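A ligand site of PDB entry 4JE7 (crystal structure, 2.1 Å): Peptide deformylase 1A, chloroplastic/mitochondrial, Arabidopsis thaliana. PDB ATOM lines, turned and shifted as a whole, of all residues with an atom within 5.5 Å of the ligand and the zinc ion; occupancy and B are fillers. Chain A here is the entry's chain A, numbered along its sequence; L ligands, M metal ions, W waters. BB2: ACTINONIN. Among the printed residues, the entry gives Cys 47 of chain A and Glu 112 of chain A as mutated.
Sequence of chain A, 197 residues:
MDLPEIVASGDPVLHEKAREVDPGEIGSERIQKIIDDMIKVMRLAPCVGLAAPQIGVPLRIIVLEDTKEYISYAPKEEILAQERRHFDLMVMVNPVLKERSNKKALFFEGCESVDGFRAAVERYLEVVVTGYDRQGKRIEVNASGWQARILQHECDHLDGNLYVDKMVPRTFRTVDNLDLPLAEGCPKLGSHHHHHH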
ATOM      1  N   PRO A  46       4.105   5.789 -22.969  1.00  0.00           N
ATOM      2  CA  PRO A  46       3.080   4.758 -23.088  1.00  0.00           C
ATOM      3  C   PRO A  46       2.825   4.126 -21.699  1.00  0.00           C
ATOM      4  O   PRO A  46       3.727   3.992 -20.855  1.00  0.00           O
ATOM      5  CB  PRO A  46       3.729   3.731 -24.052  1.00  0.00           C
ATOM      6  CG  PRO A  46       5.160   3.902 -23.866  1.00  0.00           C
ATOM      7  CD  PRO A  46       5.419   5.309 -23.458  1.00  0.00           C
ATOM      8  N   CYS A  47       1.596   3.719 -21.440  1.00  0.00           N
ATOM      9  CA  CYS A  47       1.377   2.967 -20.240  1.00  0.00           C
ATOM     10  C   CYS A  47       0.375   1.834 -20.460  1.00  0.00           C
ATOM     11  O   CYS A  47      -0.162   1.678 -21.548  1.00  0.00           O
ATOM     12  CB  CYS A  47       1.120   3.864 -19.033  1.00  0.00           C
ATOM     13  SG  CYS A  47      -0.383   4.681 -19.046  1.00  0.00           S
ATOM     14  N   VAL A  48       0.183   1.002 -19.432  1.00  0.00           N
ATOM     15  CA  VAL A  48      -0.635  -0.209 -19.557  1.00  0.00           C
ATOM     16  C   VAL A  48      -2.083  -0.108 -19.071  1.00  0.00           C
ATOM     17  O   VAL A  48      -2.813  -1.076 -19.146  1.00  0.00           O
ATOM     18  CB  VAL A  48       0.046  -1.455 -18.889  1.00  0.00           C
ATOM     19  CG1 VAL A  48       1.299  -1.864 -19.716  1.00  0.00           C
ATOM     20  CG2 VAL A  48       0.318  -1.200 -17.442  1.00  0.00           C
ATOM     21  N   GLY A  49      -2.488   1.055 -18.591  1.00  0.00           N
ATOM     22  CA  GLY A  49      -3.877   1.232 -18.178  1.00  0.00           C
ATOM     23  C   GLY A  49      -4.094   2.672 -17.822  1.00  0.00           C
ATOM     24  O   GLY A  49      -3.120   3.365 -17.626  1.00  0.00           O
ATOM     25  N   LEU A  50      -5.366   3.084 -17.717  1.00  0.00           N
ATOM     26  CA  LEU A  50      -5.739   4.467 -17.321  1.00  0.00           C
ATOM     27  C   LEU A  50      -7.111   4.509 -16.707  1.00  0.00           C
ATOM     28  O   LEU A  50      -8.012   3.721 -17.055  1.00  0.00           O
ATOM     29  CB  LEU A  50      -5.679   5.424 -18.544  1.00  0.00           C
ATOM     30  CG  LEU A  50      -5.118   6.869 -18.439  1.00  0.00           C
ATOM     31  CD1 LEU A  50      -3.541   7.007 -18.272  1.00  0.00           C
ATOM     32  CD2 LEU A  50      -5.543   7.679 -19.690  1.00  0.00           C
ATOM     33  N   ALA A  51      -7.302   5.415 -15.784  1.00  0.00           N
ATOM     34  CA  ALA A  51      -8.640   5.677 -15.290  1.00  0.00           C
ATOM     35  C   ALA A  51      -9.161   7.084 -15.658  1.00  0.00           C
ATOM     36  O   ALA A  51      -8.371   8.070 -15.787  1.00  0.00           O
ATOM     37  CB  ALA A  51      -8.701   5.438 -13.808  1.00  0.00           C
ATOM     38  N   GLN A  54      -7.888  10.413 -14.240  1.00  0.00           N
ATOM     39  CA  GLN A  54      -6.547  10.755 -14.808  1.00  0.00           C
ATOM     40  C   GLN A  54      -6.519  11.695 -16.005  1.00  0.00           C
ATOM     41  O   GLN A  54      -5.515  12.302 -16.283  1.00  0.00           O
ATOM     42  CB  GLN A  54      -5.752   9.494 -15.123  1.00  0.00           C
ATOM     43  CG  GLN A  54      -5.243   8.807 -13.868  1.00  0.00           C
ATOM     44  CD  GLN A  54      -4.491   7.550 -14.175  1.00  0.00           C
ATOM     45  OE1 GLN A  54      -5.074   6.533 -14.572  1.00  0.00           O
ATOM     46  NE2 GLN A  54      -3.162   7.620 -14.032  1.00  0.00           N
ATOM     47  N   ASP A  66      -1.657  -4.378 -22.568  1.00  0.00           N
ATOM     48  CA  ASP A  66      -0.259  -4.776 -22.415  1.00  0.00           C
ATOM     49  C   ASP A  66       0.120  -5.604 -23.613  1.00  0.00           C
ATOM     50  O   ASP A  66      -0.246  -6.775 -23.729  1.00  0.00           O
ATOM     51  CB  ASP A  66       0.002  -5.632 -21.180  1.00  0.00           C
ATOM     52  CG  ASP A  66       1.413  -5.505 -20.640  1.00  0.00           C
ATOM     53  OD1 ASP A  66       1.677  -6.077 -19.562  1.00  0.00           O
ATOM     54  OD2 ASP A  66       2.266  -4.848 -21.271  1.00  0.00           O
ATOM     55  N   TYR A  70       5.499  -3.952 -25.621  1.00  0.00           N
ATOM     56  CA  TYR A  70       5.918  -3.397 -24.341  1.00  0.00           C
ATOM     57  C   TYR A  70       6.742  -4.456 -23.569  1.00  0.00           C
ATOM     58  O   TYR A  70       7.754  -4.155 -22.925  1.00  0.00           O
ATOM     59  CB  TYR A  70       4.697  -3.032 -23.441  1.00  0.00           C
ATOM     60  CG  TYR A  70       3.725  -1.924 -23.890  1.00  0.00           C
ATOM     61  CD1 TYR A  70       4.054  -1.024 -24.911  1.00  0.00           C
ATOM     62  CD2 TYR A  70       2.496  -1.755 -23.218  1.00  0.00           C
ATOM     63  CE1 TYR A  70       3.171  -0.005 -25.306  1.00  0.00           C
ATOM     64  CE2 TYR A  70       1.611  -0.727 -23.592  1.00  0.00           C
ATOM     65  CZ  TYR A  70       1.952   0.143 -24.651  1.00  0.00           C
ATOM     66  OH  TYR A  70       1.067   1.172 -25.061  1.00  0.00           O
ATOM     67  N   ARG A  84       3.377 -11.962 -16.343  1.00  0.00           N
ATOM     68  CA  ARG A  84       3.002 -10.811 -17.147  1.00  0.00           C
ATOM     69  C   ARG A  84       2.754 -11.329 -18.578  1.00  0.00           C
ATOM     70  O   ARG A  84       3.713 -11.694 -19.295  1.00  0.00           O
ATOM     71  CB  ARG A  84       4.163  -9.820 -17.139  1.00  0.00           C
ATOM     72  CG  ARG A  84       4.089  -8.732 -18.205  1.00  0.00           C
ATOM     73  CD  ARG A  84       4.720  -7.410 -17.729  1.00  0.00           C
ATOM     74  NE  ARG A  84       4.340  -6.368 -18.628  1.00  0.00           N
ATOM     75  CZ  ARG A  84       5.026  -5.261 -18.871  1.00  0.00           C
ATOM     76  NH1 ARG A  84       6.186  -5.023 -18.219  1.00  0.00           N
ATOM     77  NH2 ARG A  84       4.540  -4.380 -19.764  1.00  0.00           N
ATOM     78  N   PHE A 108       6.985  -3.991  -7.870  1.00  0.00           N
ATOM     79  CA  PHE A 108       7.002  -2.533  -8.072  1.00  0.00           C
ATOM     80  C   PHE A 108       6.009  -2.027  -9.082  1.00  0.00           C
ATOM     81  O   PHE A 108       5.817  -2.637 -10.116  1.00  0.00           O
ATOM     82  CB  PHE A 108       8.407  -2.059  -8.468  1.00  0.00           C
ATOM     83  CG  PHE A 108       9.334  -1.959  -7.312  1.00  0.00           C
ATOM     84  CD1 PHE A 108      10.173  -3.023  -6.982  1.00  0.00           C
ATOM     85  CD2 PHE A 108       9.360  -0.839  -6.528  1.00  0.00           C
ATOM     86  CE1 PHE A 108      11.046  -2.956  -5.911  1.00  0.00           C
ATOM     87  CE2 PHE A 108      10.215  -0.772  -5.397  1.00  0.00           C
ATOM     88  CZ  PHE A 108      11.073  -1.857  -5.113  1.00  0.00           C
ATOM     89  N   GLU A 109       5.411  -0.875  -8.748  1.00  0.00           N
ATOM     90  CA  GLU A 109       4.449  -0.133  -9.613  1.00  0.00           C
ATOM     91  C   GLU A 109       4.842   1.320  -9.772  1.00  0.00           C
ATOM     92  O   GLU A 109       5.362   1.923  -8.875  1.00  0.00           O
ATOM     93  CB  GLU A 109       3.020  -0.136  -9.011  1.00  0.00           C
ATOM     94  CG  GLU A 109       2.354  -1.476  -8.829  1.00  0.00           C
ATOM     95  CD  GLU A 109       0.857  -1.359  -8.428  1.00  0.00           C
ATOM     96  OE1 GLU A 109       0.240  -0.268  -8.530  1.00  0.00           O
ATOM     97  OE2 GLU A 109       0.303  -2.420  -8.070  1.00  0.00           O
ATOM     98  N   GLY A 110       4.543   1.897 -10.923  1.00  0.00           N
ATOM     99  CA  GLY A 110       4.443   3.343 -11.011  1.00  0.00           C
ATOM    100  C   GLY A 110       3.058   3.805 -11.488  1.00  0.00           C
ATOM    101  O   GLY A 110       2.284   3.009 -12.052  1.00  0.00           O
ATOM    102  N   CYS A 111       2.783   5.091 -11.263  1.00  0.00           N
ATOM    103  CA  CYS A 111       1.535   5.710 -11.651  1.00  0.00           C
ATOM    104  C   CYS A 111       1.839   6.931 -12.520  1.00  0.00           C
ATOM    105  O   CYS A 111       2.733   7.700 -12.200  1.00  0.00           O
ATOM    106  CB  CYS A 111       0.726   6.074 -10.414  1.00  0.00           C
ATOM    107  SG  CYS A 111      -0.962   6.740 -10.709  1.00  0.00           S
ATOM    108  N   GLU A 112       1.128   7.072 -13.634  1.00  0.00           N
ATOM    109  CA  GLU A 112       1.240   8.280 -14.442  1.00  0.00           C
ATOM    110  C   GLU A 112       0.931   9.570 -13.680  1.00  0.00           C
ATOM    111  O   GLU A 112       1.322  10.667 -14.080  1.00  0.00           O
ATOM    112  CB  GLU A 112       0.338   8.188 -15.666  1.00  0.00           C
ATOM    113  CG  GLU A 112       0.973   7.337 -16.831  1.00  0.00           C
ATOM    114  CD  GLU A 112       2.412   7.717 -17.235  1.00  0.00           C
ATOM    115  OE1 GLU A 112       3.322   6.852 -17.169  1.00  0.00           O
ATOM    116  OE2 GLU A 112       2.625   8.880 -17.653  1.00  0.00           O
ATOM    117  N   SER A 113       0.207   9.447 -12.581  1.00  0.00           N
ATOM    118  CA  SER A 113      -0.170  10.602 -11.775  1.00  0.00           C
ATOM    119  C   SER A 113       0.882  10.994 -10.704  1.00  0.00           C
ATOM    120  O   SER A 113       0.803  12.076 -10.089  1.00  0.00           O
ATOM    121  CB  SER A 113      -1.543  10.354 -11.184  1.00  0.00           C
ATOM    122  OG  SER A 113      -2.472  10.282 -12.245  1.00  0.00           O
ATOM    123  N   ARG A 118       8.519   4.940  -7.860  1.00  0.00           N
ATOM    124  CA  ARG A 118       7.971   3.603  -7.863  1.00  0.00           C
ATOM    125  C   ARG A 118       7.843   3.109  -6.391  1.00  0.00           C
ATOM    126  O   ARG A 118       8.531   3.576  -5.506  1.00  0.00           O
ATOM    127  CB  ARG A 118       8.902   2.659  -8.658  1.00  0.00           C
ATOM    128  CG  ARG A 118       9.316   3.097 -10.110  1.00  0.00           C
ATOM    129  CD  ARG A 118       8.133   2.825 -11.083  1.00  0.00           C
ATOM    130  NE  ARG A 118       8.526   3.003 -12.489  1.00  0.00           N
ATOM    131  CZ  ARG A 118       8.462   4.174 -13.137  1.00  0.00           C
ATOM    132  NH1 ARG A 118       7.972   5.272 -12.529  1.00  0.00           N
ATOM    133  NH2 ARG A 118       8.908   4.264 -14.405  1.00  0.00           N
ATOM    134  N   TRP A 146      -0.215 -10.185 -13.844  1.00  0.00           N
ATOM    135  CA  TRP A 146       0.044  -8.770 -14.010  1.00  0.00           C
ATOM    136  C   TRP A 146      -1.215  -8.099 -14.445  1.00  0.00           C
ATOM    137  O   TRP A 146      -1.504  -7.006 -14.001  1.00  0.00           O
ATOM    138  CB  TRP A 146       1.089  -8.505 -15.075  1.00  0.00           C
ATOM    139  CG  TRP A 146       1.809  -7.186 -14.865  1.00  0.00           C
ATOM    140  CD1 TRP A 146       1.862  -6.144 -15.718  1.00  0.00           C
ATOM    141  CD2 TRP A 146       2.623  -6.825 -13.739  1.00  0.00           C
ATOM    142  NE1 TRP A 146       2.627  -5.115 -15.195  1.00  0.00           N
ATOM    143  CE2 TRP A 146       3.105  -5.508 -13.976  1.00  0.00           C
ATOM    144  CE3 TRP A 146       2.993  -7.489 -12.546  1.00  0.00           C
ATOM    145  CZ2 TRP A 146       3.958  -4.795 -13.047  1.00  0.00           C
ATOM    146  CZ3 TRP A 146       3.849  -6.776 -11.603  1.00  0.00           C
ATOM    147  CH2 TRP A 146       4.305  -5.447 -11.871  1.00  0.00           C
ATOM    148  N   ARG A 149      -3.238  -7.250 -11.674  1.00  0.00           N
ATOM    149  CA  ARG A 149      -2.589  -6.133 -10.991  1.00  0.00           C
ATOM    150  C   ARG A 149      -3.005  -4.832 -11.611  1.00  0.00           C
ATOM    151  O   ARG A 149      -3.391  -3.955 -10.884  1.00  0.00           O
ATOM    152  CB  ARG A 149      -1.083  -6.307 -11.030  1.00  0.00           C
ATOM    153  CG  ARG A 149      -0.216  -5.228 -10.487  1.00  0.00           C
ATOM    154  CD  ARG A 149       1.095  -5.992 -10.158  1.00  0.00           C
ATOM    155  NE  ARG A 149       1.563  -5.298  -9.033  1.00  0.00           N
ATOM    156  CZ  ARG A 149       1.856  -5.714  -7.833  1.00  0.00           C
ATOM    157  NH1 ARG A 149       1.965  -6.985  -7.453  1.00  0.00           N
ATOM    158  NH2 ARG A 149       2.126  -4.727  -7.031  1.00  0.00           N
ATOM    159  N   ILE A 150      -2.910  -4.699 -12.930  1.00  0.00           N
ATOM    160  CA  ILE A 150      -3.349  -3.464 -13.648  1.00  0.00           C
ATOM    161  C   ILE A 150      -4.805  -3.159 -13.348  1.00  0.00           C
ATOM    162  O   ILE A 150      -5.148  -2.029 -13.031  1.00  0.00           O
ATOM    163  CB  ILE A 150      -3.131  -3.600 -15.198  1.00  0.00           C
ATOM    164  CG1 ILE A 150      -1.675  -4.005 -15.530  1.00  0.00           C
ATOM    165  CG2 ILE A 150      -3.567  -2.323 -16.002  1.00  0.00           C
ATOM    166  CD1 ILE A 150      -1.510  -4.378 -17.021  1.00  0.00           C
ATOM    167  N   HIS A 153      -5.003  -1.600  -9.775  1.00  0.00           N
ATOM    168  CA  HIS A 153      -4.502  -0.229  -9.769  1.00  0.00           C
ATOM    169  C   HIS A 153      -5.522   0.765 -10.394  1.00  0.00           C
ATOM    170  O   HIS A 153      -5.770   1.863  -9.849  1.00  0.00           O
ATOM    171  CB  HIS A 153      -3.210  -0.221 -10.576  1.00  0.00           C
ATOM    172  CG  HIS A 153      -2.563   1.129 -10.712  1.00  0.00           C
ATOM    173  ND1 HIS A 153      -1.391   1.447 -10.066  1.00  0.00           N
ATOM    174  CD2 HIS A 153      -2.931   2.227 -11.411  1.00  0.00           C
ATOM    175  CE1 HIS A 153      -1.061   2.697 -10.358  1.00  0.00           C
ATOM    176  NE2 HIS A 153      -1.959   3.182 -11.191  1.00  0.00           N
ATOM    177  N   GLU A 154      -6.096   0.402 -11.547  1.00  0.00           N
ATOM    178  CA  GLU A 154      -7.075   1.243 -12.233  1.00  0.00           C
ATOM    179  C   GLU A 154      -8.374   1.396 -11.463  1.00  0.00           C
ATOM    180  O   GLU A 154      -8.861   2.522 -11.343  1.00  0.00           O
ATOM    181  CB  GLU A 154      -7.386   0.740 -13.624  1.00  0.00           C
ATOM    182  CG  GLU A 154      -6.199   0.638 -14.523  1.00  0.00           C
ATOM    183  CD  GLU A 154      -5.313   1.895 -14.524  1.00  0.00           C
ATOM    184  OE1 GLU A 154      -4.121   1.735 -14.917  1.00  0.00           O
ATOM    185  OE2 GLU A 154      -5.772   3.025 -14.165  1.00  0.00           O
ATOM    186  N   HIS A 157      -8.064   3.754  -8.622  1.00  0.00           N
ATOM    187  CA  HIS A 157      -8.160   5.164  -8.999  1.00  0.00           C
ATOM    188  C   HIS A 157      -9.604   5.673  -8.932  1.00  0.00           C
ATOM    189  O   HIS A 157      -9.852   6.856  -8.708  1.00  0.00           O
ATOM    190  CB  HIS A 157      -7.695   5.356 -10.453  1.00  0.00           C
ATOM    191  CG  HIS A 157      -6.233   5.661 -10.605  1.00  0.00           C
ATOM    192  ND1 HIS A 157      -5.640   6.795 -10.085  1.00  0.00           N
ATOM    193  CD2 HIS A 157      -5.260   5.002 -11.262  1.00  0.00           C
ATOM    194  CE1 HIS A 157      -4.369   6.817 -10.406  1.00  0.00           C
ATOM    195  NE2 HIS A 157      -4.107   5.751 -11.139  1.00  0.00           N
HETATM  196  C5  BB2 L   1      -0.554   3.785 -15.389  1.00  0.00           C
HETATM  197  C3  BB2 L   1      -1.502   4.415 -14.335  1.00  0.00           C
HETATM  198  O4  BB2 L   1      -1.130   5.273 -13.504  1.00  0.00           O
HETATM  199  N1  BB2 L   1      -2.744   3.934 -14.399  1.00  0.00           N
HETATM  200  O2  BB2 L   1      -3.719   4.379 -13.526  1.00  0.00           O
HETATM  201  C6  BB2 L   1       0.288   2.588 -14.855  1.00  0.00           C
HETATM  202  C12 BB2 L   1       1.473   2.336 -15.810  1.00  0.00           C
HETATM  203  O13 BB2 L   1       1.287   2.010 -16.987  1.00  0.00           O
HETATM  204  C7  BB2 L   1      -0.564   1.295 -14.682  1.00  0.00           C
HETATM  205  C8  BB2 L   1       0.255   0.206 -13.926  1.00  0.00           C
HETATM  206  C9  BB2 L   1      -0.615  -0.919 -13.407  1.00  0.00           C
HETATM  207  C10 BB2 L   1       0.107  -1.754 -12.302  1.00  0.00           C
HETATM  208  C11 BB2 L   1       1.438  -2.296 -12.824  1.00  0.00           C
HETATM  209  N14 BB2 L   1       2.715   2.520 -15.317  1.00  0.00           N
HETATM  210  C15 BB2 L   1       3.890   2.358 -16.173  1.00  0.00           C
HETATM  211  C16 BB2 L   1       5.151   2.868 -15.487  1.00  0.00           C
HETATM  212  C18 BB2 L   1       4.915   3.978 -14.471  1.00  0.00           C
HETATM  213  C17 BB2 L   1       5.968   1.752 -14.889  1.00  0.00           C
HETATM  214  C19 BB2 L   1       4.039   0.877 -16.648  1.00  0.00           C
HETATM  215  O20 BB2 L   1       3.744  -0.004 -15.812  1.00  0.00           O
HETATM  216  N21 BB2 L   1       4.493   0.636 -17.955  1.00  0.00           N
HETATM  217  C22 BB2 L   1       4.689  -0.697 -18.598  1.00  0.00           C
HETATM  218  C23 BB2 L   1       4.857   1.693 -18.934  1.00  0.00           C
HETATM  219  C24 BB2 L   1       4.995   1.050 -20.321  1.00  0.00           C
HETATM  220  C25 BB2 L   1       4.938  -0.454 -20.121  1.00  0.00           C
HETATM  221  C26 BB2 L   1       5.908  -1.437 -18.030  1.00  0.00           C
HETATM  222  O27 BB2 L   1       7.110  -0.617 -18.193  1.00  0.00           O
HETATM  223 ZN    ZN M   1      -2.246   5.136 -11.885  1.00  0.00          ZN
HETATM  224  O   HOH W   1       4.044  -2.616 -16.140  1.00  0.00           O
HETATM  225  O   HOH W   2       7.874  -1.228 -21.354  1.00  0.00           O
HETATM  226  O   HOH W   3       4.198   0.064 -13.117  1.00  0.00           O
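The side-chain carboxylate (OE1) of Glu 109 is in hydrogen-bond range of a ring nitrogen (ND1) of His 153 (2.8 Å). The side-chain carboxylate (OE1) of Glu 154 is in hydrogen-bond range of the backbone NH (N) of Leu 50. N of Ala 51 is in hydrogen-bond range of OE2 of Glu 154, at 3.3 Å. The side-chain amide oxygen of Gln 54 lies within hydrogen-bond range of the backbone NH of Ala 51. NE2 of Gln 54 sits at hydrogen-bond distance from OG of Ser 113. The side-chain sulfur (SG) of Cys 47 lies within hydrogen-bond range of the backbone carbonyl oxygen (O) of Gly 49 (3.4 Å). NH2 of Arg 84 lies within salt-bridge range of OD2 of Asp 66 (2.8 Å). The guanidinium group of Arg 149 lies within salt-bridge range of the side-chain carboxylate of Glu 109 (3.1 Å).
Water W1 bridges O20 of the ligand (2.6 Å) and NE1 of Trp 146 (3.0 Å). Water W3 bridges an oxygen (O20) of the ligand (2.7 Å) and the backbone NH of Gly 110 (2.9 Å). Water W2 bridges O27 of the ligand (3.3 Å) and O of Tyr 70 (3.3 Å).
The zinc ion is bound by an oxygen (O4) of the ligand (2.0 Å), a ring nitrogen (NE2) of His 153 (2.1 Å), a ring nitrogen (NE2) of His 157 (2.1 Å), an oxygen (O2) of the ligand (2.3 Å) and the side-chain sulfur of Cys 111 (2.4 Å). The zinc ion has five donor atoms within binding distance.
NE2 of Gln 54 touches the zinc ion (3.4 Å). Along chain A the residues within 4 Å of the zinc ion span positions 54 to 157.
O of Pro 46 touches C23 of the ligand, 3.2 Å away. NH1 of Arg 84 touches C26 of the ligand, at 3.6 Å. CD of Glu 109 touches C10 of the ligand, 3.97 Å away. Arg 118 touches the ligand. Trp 146 touches the ligand. Arg 149 touches the ligand. Ile 150 touches the ligand. The nearest printed residue that does not touch the ligand is Tyr 70 (4.2 Å).
The side-chain carboxylate of Glu 154 sits at hydrogen-bond distance from a nitrogen (N1) of the ligand (2.6 Å). A nitrogen (N1) of the ligand lies within hydrogen-bond range of the side-chain amide oxygen (OE1) of Gln 54 (3.5 Å). The side-chain sulfur of Cys 47 sits close to an oxygen (O13) of the ligand (3.8 Å). An oxygen (O13) of the ligand lies within hydrogen-bond range of the backbone NH (N) of Val 48. N of Glu 112 sits close to O4 of the ligand, 2.9 Å away. The backbone carbonyl oxygen (O) of Gly 49 sits at hydrogen-bond distance from a nitrogen (N1) of the ligand. The backbone carbonyl oxygen (O) of Gly 110 sits at hydrogen-bond distance from a nitrogen (N14) of the ligand.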
